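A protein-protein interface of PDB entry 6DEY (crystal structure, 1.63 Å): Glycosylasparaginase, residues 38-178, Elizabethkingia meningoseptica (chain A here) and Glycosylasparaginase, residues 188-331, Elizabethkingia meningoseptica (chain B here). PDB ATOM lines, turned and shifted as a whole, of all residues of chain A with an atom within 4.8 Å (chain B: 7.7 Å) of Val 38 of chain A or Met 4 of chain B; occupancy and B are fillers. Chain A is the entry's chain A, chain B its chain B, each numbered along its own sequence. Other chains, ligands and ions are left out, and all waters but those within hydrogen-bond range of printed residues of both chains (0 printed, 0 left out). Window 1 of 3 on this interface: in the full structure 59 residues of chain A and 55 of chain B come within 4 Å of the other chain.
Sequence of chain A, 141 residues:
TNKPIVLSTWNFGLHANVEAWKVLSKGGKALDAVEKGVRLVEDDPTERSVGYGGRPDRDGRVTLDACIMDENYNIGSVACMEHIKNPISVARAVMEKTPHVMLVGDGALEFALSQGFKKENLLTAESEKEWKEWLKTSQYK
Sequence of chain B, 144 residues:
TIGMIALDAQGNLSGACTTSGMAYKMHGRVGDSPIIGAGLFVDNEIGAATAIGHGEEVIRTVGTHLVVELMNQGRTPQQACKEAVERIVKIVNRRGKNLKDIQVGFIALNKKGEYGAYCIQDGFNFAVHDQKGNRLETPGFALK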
ATOM      1  N   VAL A   6     -17.489  15.276 -21.324  1.00  0.00           N
ATOM      2  CA  VAL A   6     -18.888  15.308 -21.838  1.00  0.00           C
ATOM      3  C   VAL A   6     -19.060  14.254 -22.868  1.00  0.00           C
ATOM      4  O   VAL A   6     -18.152  14.032 -23.706  1.00  0.00           O
ATOM      5  CB  VAL A   6     -19.283  16.697 -22.375  1.00  0.00           C
ATOM      6  CG1 VAL A   6     -18.337  17.218 -23.462  1.00  0.00           C
ATOM      7  CG2 VAL A   6     -20.658  16.758 -22.963  1.00  0.00           C
ATOM      8  N   LEU A   7     -20.228  13.588 -22.868  1.00  0.00           N
ATOM      9  CA  LEU A   7     -20.633  12.596 -23.874  1.00  0.00           C
ATOM     10  C   LEU A   7     -21.944  13.026 -24.476  1.00  0.00           C
ATOM     11  O   LEU A   7     -22.822  13.547 -23.766  1.00  0.00           O
ATOM     12  CB  LEU A   7     -20.883  11.210 -23.270  1.00  0.00           C
ATOM     13  CG  LEU A   7     -19.675  10.238 -23.220  1.00  0.00           C
ATOM     14  CD1 LEU A   7     -18.675  10.721 -22.258  1.00  0.00           C
ATOM     15  CD2 LEU A   7     -20.157   8.815 -22.918  1.00  0.00           C
ATOM     16  N   SER A   8     -22.107  12.796 -25.764  1.00  0.00           N
ATOM     17  CA  SER A   8     -23.379  13.106 -26.390  1.00  0.00           C
ATOM     18  C   SER A   8     -23.619  12.149 -27.527  1.00  0.00           C
ATOM     19  O   SER A   8     -22.699  11.450 -27.971  1.00  0.00           O
ATOM     20  CB  SER A   8     -23.526  14.522 -26.792  1.00  0.00           C
ATOM     21  OG  SER A   8     -22.585  14.837 -27.808  1.00  0.00           O
ATOM     22  N   ALA A  16     -21.973  19.354 -30.821  1.00  0.00           N
ATOM     23  CA  ALA A  16     -22.544  19.830 -29.554  1.00  0.00           C
ATOM     24  C   ALA A  16     -21.444  19.871 -28.529  1.00  0.00           C
ATOM     25  O   ALA A  16     -21.455  20.793 -27.673  1.00  0.00           O
ATOM     26  CB  ALA A  16     -23.687  18.863 -29.164  1.00  0.00           C
ATOM     27  N   ASN A  17     -20.617  18.788 -28.527  1.00  0.00           N
ATOM     28  CA  ASN A  17     -19.561  18.694 -27.498  1.00  0.00           C
ATOM     29  C   ASN A  17     -18.636  19.903 -27.487  1.00  0.00           C
ATOM     30  O   ASN A  17     -18.143  20.310 -26.408  1.00  0.00           O
ATOM     31  CB  ASN A  17     -18.700  17.467 -27.652  1.00  0.00           C
ATOM     32  CG  ASN A  17     -19.320  16.225 -27.093  1.00  0.00           C
ATOM     33  OD1 ASN A  17     -20.479  16.204 -26.578  1.00  0.00           O
ATOM     34  ND2 ASN A  17     -18.547  15.127 -27.158  1.00  0.00           N
ATOM     35  N   ALA A  20     -20.347  22.563 -25.536  1.00  0.00           N
ATOM     36  CA  ALA A  20     -20.293  22.232 -24.121  1.00  0.00           C
ATOM     37  C   ALA A  20     -18.904  22.487 -23.507  1.00  0.00           C
ATOM     38  O   ALA A  20     -18.781  22.964 -22.392  1.00  0.00           O
ATOM     39  CB  ALA A  20     -20.733  20.783 -23.912  1.00  0.00           C
ATOM     40  N   ALA A  33     -23.186  23.659 -19.405  1.00  0.00           N
ATOM     41  CA  ALA A  33     -22.527  23.076 -20.573  1.00  0.00           C
ATOM     42  C   ALA A  33     -23.517  22.241 -21.342  1.00  0.00           C
ATOM     43  O   ALA A  33     -23.514  22.307 -22.596  1.00  0.00           O
ATOM     44  CB  ALA A  33     -21.428  22.207 -20.095  1.00  0.00           C
ATOM     45  N   VAL A  34     -24.301  21.419 -20.656  1.00  0.00           N
ATOM     46  CA  VAL A  34     -25.234  20.574 -21.420  1.00  0.00           C
ATOM     47  C   VAL A  34     -26.335  21.354 -22.104  1.00  0.00           C
ATOM     48  O   VAL A  34     -26.808  21.004 -23.216  1.00  0.00           O
ATOM     49  CB  VAL A  34     -25.713  19.351 -20.649  1.00  0.00           C
ATOM     50  CG1 VAL A  34     -24.556  18.487 -20.168  1.00  0.00           C
ATOM     51  CG2 VAL A  34     -26.648  19.740 -19.472  1.00  0.00           C
ATOM     52  N   GLU A  35     -26.823  22.404 -21.475  1.00  0.00           N
ATOM     53  CA  GLU A  35     -27.826  23.240 -22.104  1.00  0.00           C
ATOM     54  C   GLU A  35     -27.253  23.924 -23.366  1.00  0.00           C
ATOM     55  O   GLU A  35     -27.896  23.855 -24.412  1.00  0.00           O
ATOM     56  CB  GLU A  35     -28.335  24.273 -21.137  1.00  0.00           C
ATOM     57  CG  GLU A  35     -29.390  25.204 -21.785  1.00  0.00           C
ATOM     58  CD  GLU A  35     -29.883  26.284 -20.913  1.00  0.00           C
ATOM     59  OE1 GLU A  35     -29.108  26.653 -20.020  1.00  0.00           O
ATOM     60  OE2 GLU A  35     -30.987  26.900 -21.138  1.00  0.00           O
ATOM     61  N   LYS A  36     -26.087  24.554 -23.228  1.00  0.00           N
ATOM     62  CA  LYS A  36     -25.439  25.117 -24.434  1.00  0.00           C
ATOM     63  C   LYS A  36     -25.187  24.111 -25.519  1.00  0.00           C
ATOM     64  O   LYS A  36     -25.368  24.407 -26.744  1.00  0.00           O
ATOM     65  CB  LYS A  36     -24.155  25.868 -24.057  1.00  0.00           C
ATOM     66  CG  LYS A  36     -24.441  27.161 -23.266  1.00  0.00           C
ATOM     67  CD  LYS A  36     -25.229  28.195 -24.032  1.00  0.00           C
ATOM     68  CE  LYS A  36     -24.691  29.629 -23.904  1.00  0.00           C
ATOM     69  NZ  LYS A  36     -24.930  30.102 -22.505  1.00  0.00           N
ATOM     70  N   GLY A  37     -24.740  22.944 -25.138  1.00  0.00           N
ATOM     71  CA  GLY A  37     -24.409  21.943 -26.105  1.00  0.00           C
ATOM     72  C   GLY A  37     -25.607  21.535 -26.957  1.00  0.00           C
ATOM     73  O   GLY A  37     -25.504  21.475 -28.220  1.00  0.00           O
ATOM     74  N   VAL A  38     -26.731  21.235 -26.299  1.00  0.00           N
ATOM     75  CA  VAL A  38     -27.875  20.695 -27.073  1.00  0.00           C
ATOM     76  C   VAL A  38     -28.603  21.817 -27.807  1.00  0.00           C
ATOM     77  O   VAL A  38     -29.199  21.558 -28.847  1.00  0.00           O
ATOM     78  CB  VAL A  38     -28.836  19.779 -26.291  1.00  0.00           C
ATOM     79  CG1 VAL A  38     -28.084  18.630 -25.638  1.00  0.00           C
ATOM     80  CG2 VAL A  38     -29.582  20.548 -25.245  1.00  0.00           C
ATOM     81  N   ARG A  39     -28.492  23.051 -27.303  1.00  0.00           N
ATOM     82  CA  ARG A  39     -29.149  24.172 -28.006  1.00  0.00           C
ATOM     83  C   ARG A  39     -28.540  24.323 -29.389  1.00  0.00           C
ATOM     84  O   ARG A  39     -29.274  24.765 -30.286  1.00  0.00           O
ATOM     85  CB  ARG A  39     -28.962  25.475 -27.214  1.00  0.00           C
ATOM     86  CG  ARG A  39     -29.966  25.692 -26.081  1.00  0.00           C
ATOM     87  CD  ARG A  39     -29.673  26.943 -25.260  1.00  0.00           C
ATOM     88  NE  ARG A  39     -29.830  28.086 -26.155  1.00  0.00           N
ATOM     89  CZ  ARG A  39     -30.861  28.891 -26.237  1.00  0.00           C
ATOM     90  NH1 ARG A  39     -30.875  29.865 -27.192  1.00  0.00           N
ATOM     91  NH2 ARG A  39     -31.937  28.775 -25.488  1.00  0.00           N
ATOM     92  N   LEU A  40     -27.285  24.032 -29.605  1.00  0.00           N
ATOM     93  CA  LEU A  40     -26.689  24.095 -30.972  1.00  0.00           C
ATOM     94  C   LEU A  40     -27.508  23.291 -31.948  1.00  0.00           C
ATOM     95  O   LEU A  40     -27.796  23.718 -33.065  1.00  0.00           O
ATOM     96  CB  LEU A  40     -25.232  23.616 -30.911  1.00  0.00           C
ATOM     97  CG  LEU A  40     -24.530  23.697 -32.293  1.00  0.00           C
ATOM     98  CD1 LEU A  40     -24.096  25.143 -32.612  1.00  0.00           C
ATOM     99  CD2 LEU A  40     -23.383  22.668 -32.282  1.00  0.00           C
ATOM    100  N   VAL A  41     -27.916  22.111 -31.548  1.00  0.00           N
ATOM    101  CA  VAL A  41     -28.605  21.197 -32.442  1.00  0.00           C
ATOM    102  C   VAL A  41     -30.066  21.585 -32.590  1.00  0.00           C
ATOM    103  O   VAL A  41     -30.643  21.481 -33.688  1.00  0.00           O
ATOM    104  CB  VAL A  41     -28.385  19.785 -31.933  1.00  0.00           C
ATOM    105  CG1 VAL A  41     -28.953  18.779 -32.881  1.00  0.00           C
ATOM    106  CG2 VAL A  41     -26.907  19.544 -31.853  1.00  0.00           C
ATOM    107  N   GLU A  42     -30.705  22.084 -31.535  1.00  0.00           N
ATOM    108  CA  GLU A  42     -32.018  22.663 -31.612  1.00  0.00           C
ATOM    109  C   GLU A  42     -32.016  23.800 -32.631  1.00  0.00           C
ATOM    110  O   GLU A  42     -32.982  23.958 -33.334  1.00  0.00           O
ATOM    111  CB  GLU A  42     -32.420  23.216 -30.199  1.00  0.00           C
ATOM    112  CG  GLU A  42     -32.720  22.164 -29.147  1.00  0.00           C
ATOM    113  CD  GLU A  42     -33.116  22.774 -27.851  1.00  0.00           C
ATOM    114  OE1 GLU A  42     -32.698  23.906 -27.548  1.00  0.00           O
ATOM    115  OE2 GLU A  42     -33.715  22.023 -27.033  1.00  0.00           O
ATOM    116  N   VAL A  50     -34.139  17.287 -34.066  1.00  0.00           N
ATOM    117  CA  VAL A  50     -34.068  18.087 -32.839  1.00  0.00           C
ATOM    118  C   VAL A  50     -34.499  19.493 -33.209  1.00  0.00           C
ATOM    119  O   VAL A  50     -33.931  20.068 -34.135  1.00  0.00           O
ATOM    120  CB  VAL A  50     -32.619  18.117 -32.258  1.00  0.00           C
ATOM    121  CG1 VAL A  50     -32.509  18.939 -30.990  1.00  0.00           C
ATOM    122  CG2 VAL A  50     -32.101  16.709 -31.989  1.00  0.00           C
ATOM    123  N   ILE A  88     -35.099  22.745 -24.508  1.00  0.00           N
ATOM    124  CA  ILE A  88     -34.235  22.455 -23.303  1.00  0.00           C
ATOM    125  C   ILE A  88     -34.241  23.617 -22.347  1.00  0.00           C
ATOM    126  O   ILE A  88     -34.182  23.459 -21.128  1.00  0.00           O
ATOM    127  CB  ILE A  88     -32.793  22.070 -23.715  1.00  0.00           C
ATOM    128  CG1 ILE A  88     -32.054  21.417 -22.535  1.00  0.00           C
ATOM    129  CG2 ILE A  88     -32.013  23.271 -24.244  1.00  0.00           C
ATOM    130  CD1 ILE A  88     -32.684  20.174 -22.020  1.00  0.00           C
ATOM    131  N   THR B   1     -33.126  13.045 -31.978  1.00  0.00           N
ATOM    132  CA  THR B   1     -32.828  13.276 -30.512  1.00  0.00           C
ATOM    133  C   THR B   1     -31.347  13.515 -30.284  1.00  0.00           C
ATOM    134  O   THR B   1     -30.503  12.893 -30.911  1.00  0.00           O
ATOM    135  CB  THR B   1     -33.166  11.990 -29.703  1.00  0.00           C
ATOM    136  OG1 THR B   1     -34.546  11.657 -29.955  1.00  0.00           O
ATOM    137  CG2 THR B   1     -32.990  12.229 -28.236  1.00  0.00           C
ATOM    138  N   ILE B   2     -31.008  14.404 -29.349  1.00  0.00           N
ATOM    139  CA  ILE B   2     -29.693  14.479 -28.789  1.00  0.00           C
ATOM    140  C   ILE B   2     -29.791  14.356 -27.292  1.00  0.00           C
ATOM    141  O   ILE B   2     -30.630  15.053 -26.663  1.00  0.00           O
ATOM    142  CB  ILE B   2     -28.887  15.735 -29.186  1.00  0.00           C
ATOM    143  CG1 ILE B   2     -27.425  15.591 -28.652  1.00  0.00           C
ATOM    144  CG2 ILE B   2     -29.542  17.063 -28.782  1.00  0.00           C
ATOM    145  CD1 ILE B   2     -26.489  16.688 -29.138  1.00  0.00           C
ATOM    146  N   GLY B   3     -28.904  13.547 -26.744  1.00  0.00           N
ATOM    147  CA  GLY B   3     -28.783  13.424 -25.284  1.00  0.00           C
ATOM    148  C   GLY B   3     -27.392  13.822 -24.976  1.00  0.00           C
ATOM    149  O   GLY B   3     -26.447  13.471 -25.754  1.00  0.00           O
ATOM    150  N   MET B   4     -27.127  14.492 -23.842  1.00  0.00           N
ATOM    151  CA  MET B   4     -25.749  14.909 -23.493  1.00  0.00           C
ATOM    152  C   MET B   4     -25.650  14.783 -21.937  1.00  0.00           C
ATOM    153  O   MET B   4     -26.580  15.292 -21.244  1.00  0.00           O
ATOM    154  CB  MET B   4     -25.511  16.361 -23.916  1.00  0.00           C
ATOM    155  CG  MET B   4     -24.182  16.842 -23.514  1.00  0.00           C
ATOM    156  SD  MET B   4     -23.792  18.503 -24.157  1.00  0.00           S
ATOM    157  CE  MET B   4     -23.221  18.132 -25.836  1.00  0.00           C
ATOM    158  N   ILE B   5     -24.522  14.225 -21.473  1.00  0.00           N
ATOM    159  CA  ILE B   5     -24.204  14.136 -20.029  1.00  0.00           C
ATOM    160  C   ILE B   5     -22.804  14.614 -19.840  1.00  0.00           C
ATOM    161  O   ILE B   5     -21.946  14.336 -20.669  1.00  0.00           O
ATOM    162  CB  ILE B   5     -24.456  12.650 -19.527  1.00  0.00           C
ATOM    163  CG1 ILE B   5     -23.629  11.641 -20.364  1.00  0.00           C
ATOM    164  CG2 ILE B   5     -25.974  12.326 -19.524  1.00  0.00           C
ATOM    165  CD1 ILE B   5     -23.811  10.206 -19.860  1.00  0.00           C
ATOM    166  N   ALA B   6     -22.586  15.333 -18.742  1.00  0.00           N
ATOM    167  CA  ALA B   6     -21.254  15.878 -18.478  1.00  0.00           C
ATOM    168  C   ALA B   6     -20.934  15.786 -17.015  1.00  0.00           C
ATOM    169  O   ALA B   6     -21.829  15.853 -16.157  1.00  0.00           O
ATOM    170  CB  ALA B   6     -21.168  17.310 -18.947  1.00  0.00           C
ATOM    171  N   SER B  14     -24.414  16.615 -14.777  1.00  0.00           N
ATOM    172  CA  SER B  14     -25.743  17.095 -15.244  1.00  0.00           C
ATOM    173  C   SER B  14     -26.037  16.479 -16.594  1.00  0.00           C
ATOM    174  O   SER B  14     -25.092  15.941 -17.282  1.00  0.00           O
ATOM    175  CB  SER B  14     -25.803  18.614 -15.284  1.00  0.00           C
ATOM    176  OG  SER B  14     -25.719  19.159 -13.980  1.00  0.00           O
ATOM    177  N   GLY B  15     -27.270  16.602 -17.040  1.00  0.00           N
ATOM    178  CA  GLY B  15     -27.592  16.138 -18.395  1.00  0.00           C
ATOM    179  C   GLY B  15     -28.779  16.795 -19.001  1.00  0.00           C
ATOM    180  O   GLY B  15     -29.560  17.434 -18.349  1.00  0.00           O
ATOM    181  N   ALA B  16     -28.901  16.586 -20.321  1.00  0.00           N
ATOM    182  CA  ALA B  16     -29.934  17.210 -21.071  1.00  0.00           C
ATOM    183  C   ALA B  16     -30.339  16.317 -22.253  1.00  0.00           C
ATOM    184  O   ALA B  16     -29.497  15.642 -22.790  1.00  0.00           O
ATOM    185  CB  ALA B  16     -29.413  18.516 -21.647  1.00  0.00           C
ATOM    186  N   CYS B  17     -31.624  16.317 -22.624  1.00  0.00           N
ATOM    187  CA  CYS B  17     -32.116  15.537 -23.780  1.00  0.00           C
ATOM    188  C   CYS B  17     -33.093  16.394 -24.504  1.00  0.00           C
ATOM    189  O   CYS B  17     -33.911  16.993 -23.847  1.00  0.00           O
ATOM    190  CB  CYS B  17     -32.933  14.347 -23.252  1.00  0.00           C
ATOM    191  SG  CYS B  17     -32.037  13.008 -22.624  1.00  0.00           S
ATOM    192  N   THR B  18     -33.107  16.385 -25.822  1.00  0.00           N
ATOM    193  CA  THR B  18     -34.046  17.176 -26.557  1.00  0.00           C
ATOM    194  C   THR B  18     -34.302  16.578 -27.924  1.00  0.00           C
ATOM    195  O   THR B  18     -33.378  16.068 -28.535  1.00  0.00           O
ATOM    196  CB  THR B  18     -33.499  18.595 -26.640  1.00  0.00           C
ATOM    197  OG1 THR B  18     -34.450  19.404 -27.372  1.00  0.00           O
ATOM    198  CG2 THR B  18     -32.196  18.733 -27.171  1.00  0.00           C
ATOM    199  N   GLY B  39     -35.364   8.593 -20.880  1.00  0.00           N
ATOM    200  CA  GLY B  39     -34.375   9.222 -21.693  1.00  0.00           C
ATOM    201  C   GLY B  39     -33.098   9.703 -21.021  1.00  0.00           C
ATOM    202  O   GLY B  39     -32.026   9.788 -21.650  1.00  0.00           O
ATOM    203  N   LEU B  40     -33.260  10.061 -19.735  1.00  0.00           N
ATOM    204  CA  LEU B  40     -32.142  10.728 -19.003  1.00  0.00           C
ATOM    205  C   LEU B  40     -32.260  10.439 -17.523  1.00  0.00           C
ATOM    206  O   LEU B  40     -33.350  10.506 -16.940  1.00  0.00           O
ATOM    207  CB  LEU B  40     -32.286  12.209 -19.177  1.00  0.00           C
ATOM    208  CG  LEU B  40     -31.265  13.100 -18.469  1.00  0.00           C
ATOM    209  CD1 LEU B  40     -29.851  12.821 -18.979  1.00  0.00           C
ATOM    210  CD2 LEU B  40     -31.598  14.587 -18.568  1.00  0.00           C
ATOM    211  N   VAL B  42     -29.686  11.213 -13.824  1.00  0.00           N
ATOM    212  CA  VAL B  42     -28.455  11.733 -13.279  1.00  0.00           C
ATOM    213  C   VAL B  42     -28.556  11.622 -11.734  1.00  0.00           C
ATOM    214  O   VAL B  42     -29.466  12.185 -11.106  1.00  0.00           O
ATOM    215  CB  VAL B  42     -28.245  13.182 -13.620  1.00  0.00           C
ATOM    216  CG1 VAL B  42     -26.963  13.694 -12.920  1.00  0.00           C
ATOM    217  CG2 VAL B  42     -28.191  13.410 -15.127  1.00  0.00           C
ATOM    218  N   ALA B  48     -24.488   9.088 -14.514  1.00  0.00           N
ATOM    219  CA  ALA B  48     -25.528   9.590 -15.415  1.00  0.00           C
ATOM    220  C   ALA B  48     -25.630   8.745 -16.622  1.00  0.00           C
ATOM    221  O   ALA B  48     -24.666   8.050 -17.038  1.00  0.00           O
ATOM    222  CB  ALA B  48     -25.235  10.997 -15.810  1.00  0.00           C
ATOM    223  N   ALA B  49     -26.792   8.716 -17.255  1.00  0.00           N
ATOM    224  CA  ALA B  49     -27.016   7.949 -18.481  1.00  0.00           C
ATOM    225  C   ALA B  49     -28.023   8.667 -19.384  1.00  0.00           C
ATOM    226  O   ALA B  49     -28.946   9.321 -18.850  1.00  0.00           O
ATOM    227  CB  ALA B  49     -27.411   6.577 -18.236  1.00  0.00           C
ATOM    228  N   THR B  50     -27.911   8.509 -20.697  1.00  0.00           N
ATOM    229  CA  THR B  50     -28.932   8.991 -21.586  1.00  0.00           C
ATOM    230  C   THR B  50     -29.093   7.919 -22.626  1.00  0.00           C
ATOM    231  O   THR B  50     -28.178   7.170 -22.901  1.00  0.00           O
ATOM    232  CB  THR B  50     -28.655  10.475 -22.057  1.00  0.00           C
ATOM    233  OG1 THR B  50     -29.827  10.992 -22.653  1.00  0.00           O
ATOM    234  CG2 THR B  50     -27.485  10.604 -23.001  1.00  0.00           C
ATOM    235  N   ALA B  51     -30.268   7.879 -23.235  1.00  0.00           N
ATOM    236  CA  ALA B  51     -30.690   6.793 -24.119  1.00  0.00           C
ATOM    237  C   ALA B  51     -30.835   7.169 -25.583  1.00  0.00           C
ATOM    238  O   ALA B  51     -31.181   8.299 -25.923  1.00  0.00           O
ATOM    239  CB  ALA B  51     -32.071   6.271 -23.711  1.00  0.00           C
ATOM    240  N   ILE B 107     -25.563   5.652 -23.319  1.00  0.00           N
ATOM    241  CA  ILE B 107     -24.211   6.178 -22.995  1.00  0.00           C
ATOM    242  C   ILE B 107     -24.269   6.509 -21.516  1.00  0.00           C
ATOM    243  O   ILE B 107     -25.297   6.939 -21.001  1.00  0.00           O
ATOM    244  CB  ILE B 107     -23.802   7.380 -23.825  1.00  0.00           C
ATOM    245  CG1 ILE B 107     -24.659   8.621 -23.686  1.00  0.00           C
ATOM    246  CG2 ILE B 107     -23.661   7.028 -25.344  1.00  0.00           C
ATOM    247  CD1 ILE B 107     -24.227   9.810 -24.535  1.00  0.00           C
ATOM    248  N   LEU B 109     -21.843   7.755 -17.783  1.00  0.00           N
ATOM    249  CA  LEU B 109     -20.691   8.368 -17.151  1.00  0.00           C
ATOM    250  C   LEU B 109     -20.791   8.075 -15.647  1.00  0.00           C
ATOM    251  O   LEU B 109     -21.922   8.007 -15.087  1.00  0.00           O
ATOM    252  CB  LEU B 109     -20.775   9.873 -17.414  1.00  0.00           C
ATOM    253  CG  LEU B 109     -19.750  10.874 -17.494  1.00  0.00           C
ATOM    254  CD1 LEU B 109     -18.466  10.334 -18.153  1.00  0.00           C
ATOM    255  CD2 LEU B 109     -20.324  12.139 -18.109  1.00  0.00           C
ATOM    256  N   ALA B 127     -20.213  10.811 -29.147  1.00  0.00           N
ATOM    257  CA  ALA B 127     -19.055  11.744 -29.109  1.00  0.00           C
ATOM    258  C   ALA B 127     -18.630  11.935 -27.688  1.00  0.00           C
ATOM    259  O   ALA B 127     -19.498  12.128 -26.794  1.00  0.00           O
ATOM    260  CB  ALA B 127     -19.409  13.062 -29.693  1.00  0.00           C
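The backbone NH (N) of Thr 18 of chain B is in hydrogen-bond range of the backbone carbonyl oxygen (O) of Ile 2 of chain B, at 2.9 Å.
N of Ala 16 of chain B lies within hydrogen-bond range of O of Met 4 of chain B (2.8 Å).
O of Ser 14 of chain B is in hydrogen-bond range of N of Ala 6 of chain B (3.0 Å).
O of Gly 39 of chain B is in hydrogen-bond range of SG of Cys 17 of chain B, at 3.4 Å.
OG1 of Thr 50 of chain B is in hydrogen-bond range of SG of Cys 17 of chain B.
O of Thr 50 of chain B is in hydrogen-bond range of N of Ile 107 of chain B (3.1 Å).
The backbone carbonyl oxygen (O) of Ile 5 of chain B lies within hydrogen-bond range of the backbone NH (N) of Leu 7 of chain A (2.9 Å).
The backbone NH (N) of Ala 127 of chain B lies within hydrogen-bond range of the backbone carbonyl oxygen (O) of Ser 8 of chain A.
The backbone carbonyl oxygen of Ala 127 of chain B lies within hydrogen-bond range of the side-chain amide nitrogen of Asn 17 of chain A (3.2 Å).
The side-chain hydroxyl (OG1) of Thr 18 of chain B is in hydrogen-bond range of the side-chain carboxylate (OE2) of Glu 42 of chain A.
Val 38 of chain A touches just these residues of chain B: Ile 2 (3.8 Å), Met 4 (3.8 Å) and Thr 18 (3.6 Å).
Printed residues of chain A within 4 Å of Met 4 of chain B: Val 6 (3.6 Å), Leu 7 (3.2 Å), Ser 8 (3.7 Å), Ala 16 (3.4 Å), Asn 17 (3.4 Å), Ala 20 (3.8 Å), Val 34 (3.7 Å) and Val 38 (3.8 Å).
Printed residues of chain A within 4 Å of Ser 14 of chain B: Val 34 (3.9 Å).
Of the printed residues of chain A, Thr 18 of chain B touches Val 38 (3.6 Å), Glu 42 (2.7 Å) and Val 50 (3.7 Å).
Leu 40 of chain B touches none of the printed residues of chain A.
The nearest printed residue of chain B that does not touch Asn 17 of chain A is Ile 2 of chain B (6.3 Å).
Among the printed residues, merely in contact across the chains: Val 6 of chain A with Met 4 of chain B (3.6 Å), Val 6 of chain A with Ile 5 of chain B (3.4 Å), Val 6 of chain A with Ala 6 of chain B (3.96 Å), Val 6 of chain A with Ala 127 of chain B (3.9 Å), Leu 7 of chain A with Met 4 of chain B (3.2 Å), Leu 7 of chain A with Ile 107 of chain B (3.8 Å), Leu 7 of chain A with Ala 127 of chain B (3.2 Å), Ser 8 of chain A with Gly 3 of chain B (3.2 Å), Ser 8 of chain A with Met 4 of chain B (3.7 Å), Ser 8 of chain A with Ile 107 of chain B (3.8 Å), Ala 16 of chain A with Ile 2 of chain B (3.5 Å), Ala 16 of chain A with Met 4 of chain B (3.4 Å), Asn 17 of chain A with Met 4 of chain B (3.4 Å), Ala 20 of chain A with Met 4 of chain B (3.8 Å), Val 34 of chain A with Met 4 of chain B (3.7 Å), Val 34 of chain A with Ala 6 of chain B (3.8 Å), Val 34 of chain A with Ser 14 of chain B (3.9 Å), Val 34 of chain A with Gly 15 of chain B (3.7 Å), Val 34 of chain A with Ala 16 of chain B (3.7 Å), Val 38 of chain A with Ile 2 of chain B (3.8 Å), Val 38 of chain A with Met 4 of chain B (3.8 Å), Val 38 of chain A with Thr 18 of chain B (3.6 Å), Val 41 of chain A with Ile 2 of chain B (3.96 Å), Val 50 of chain A with Thr 1 of chain B (3.7 Å), Val 50 of chain A with Ile 2 of chain B (3.7 Å), Val 50 of chain A with Thr 18 of chain B (3.7 Å), Ile 88 of chain A with Ala 16 of chain B (3.7 Å) and Ile 88 of chain A with Cys 17 of chain B (3.9 Å).
Of the 18 printed residues of chain A, 12 touch a printed residue of chain B.
Printed residues of chain A that touch a printed residue of chain B: Val 6, Leu 7, Ser 8, Ala 16, Asn 17, Ala 20, Val 34, Val 38, Val 41, Glu 42, Val 50 and Ile 88.
Along chain A the printed residues that touch a printed residue of chain B span positions 6 to 88.
Hydrophobic or aromatic side chains of chain B within 4 Å of the printed part of chain A: Ile 2, Met 4, Ile 5, Ala 6, Ala 16, Ile 107 and Ala 127.
Along chain B the printed residues that touch a printed residue of chain A span positions 1 to 127.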
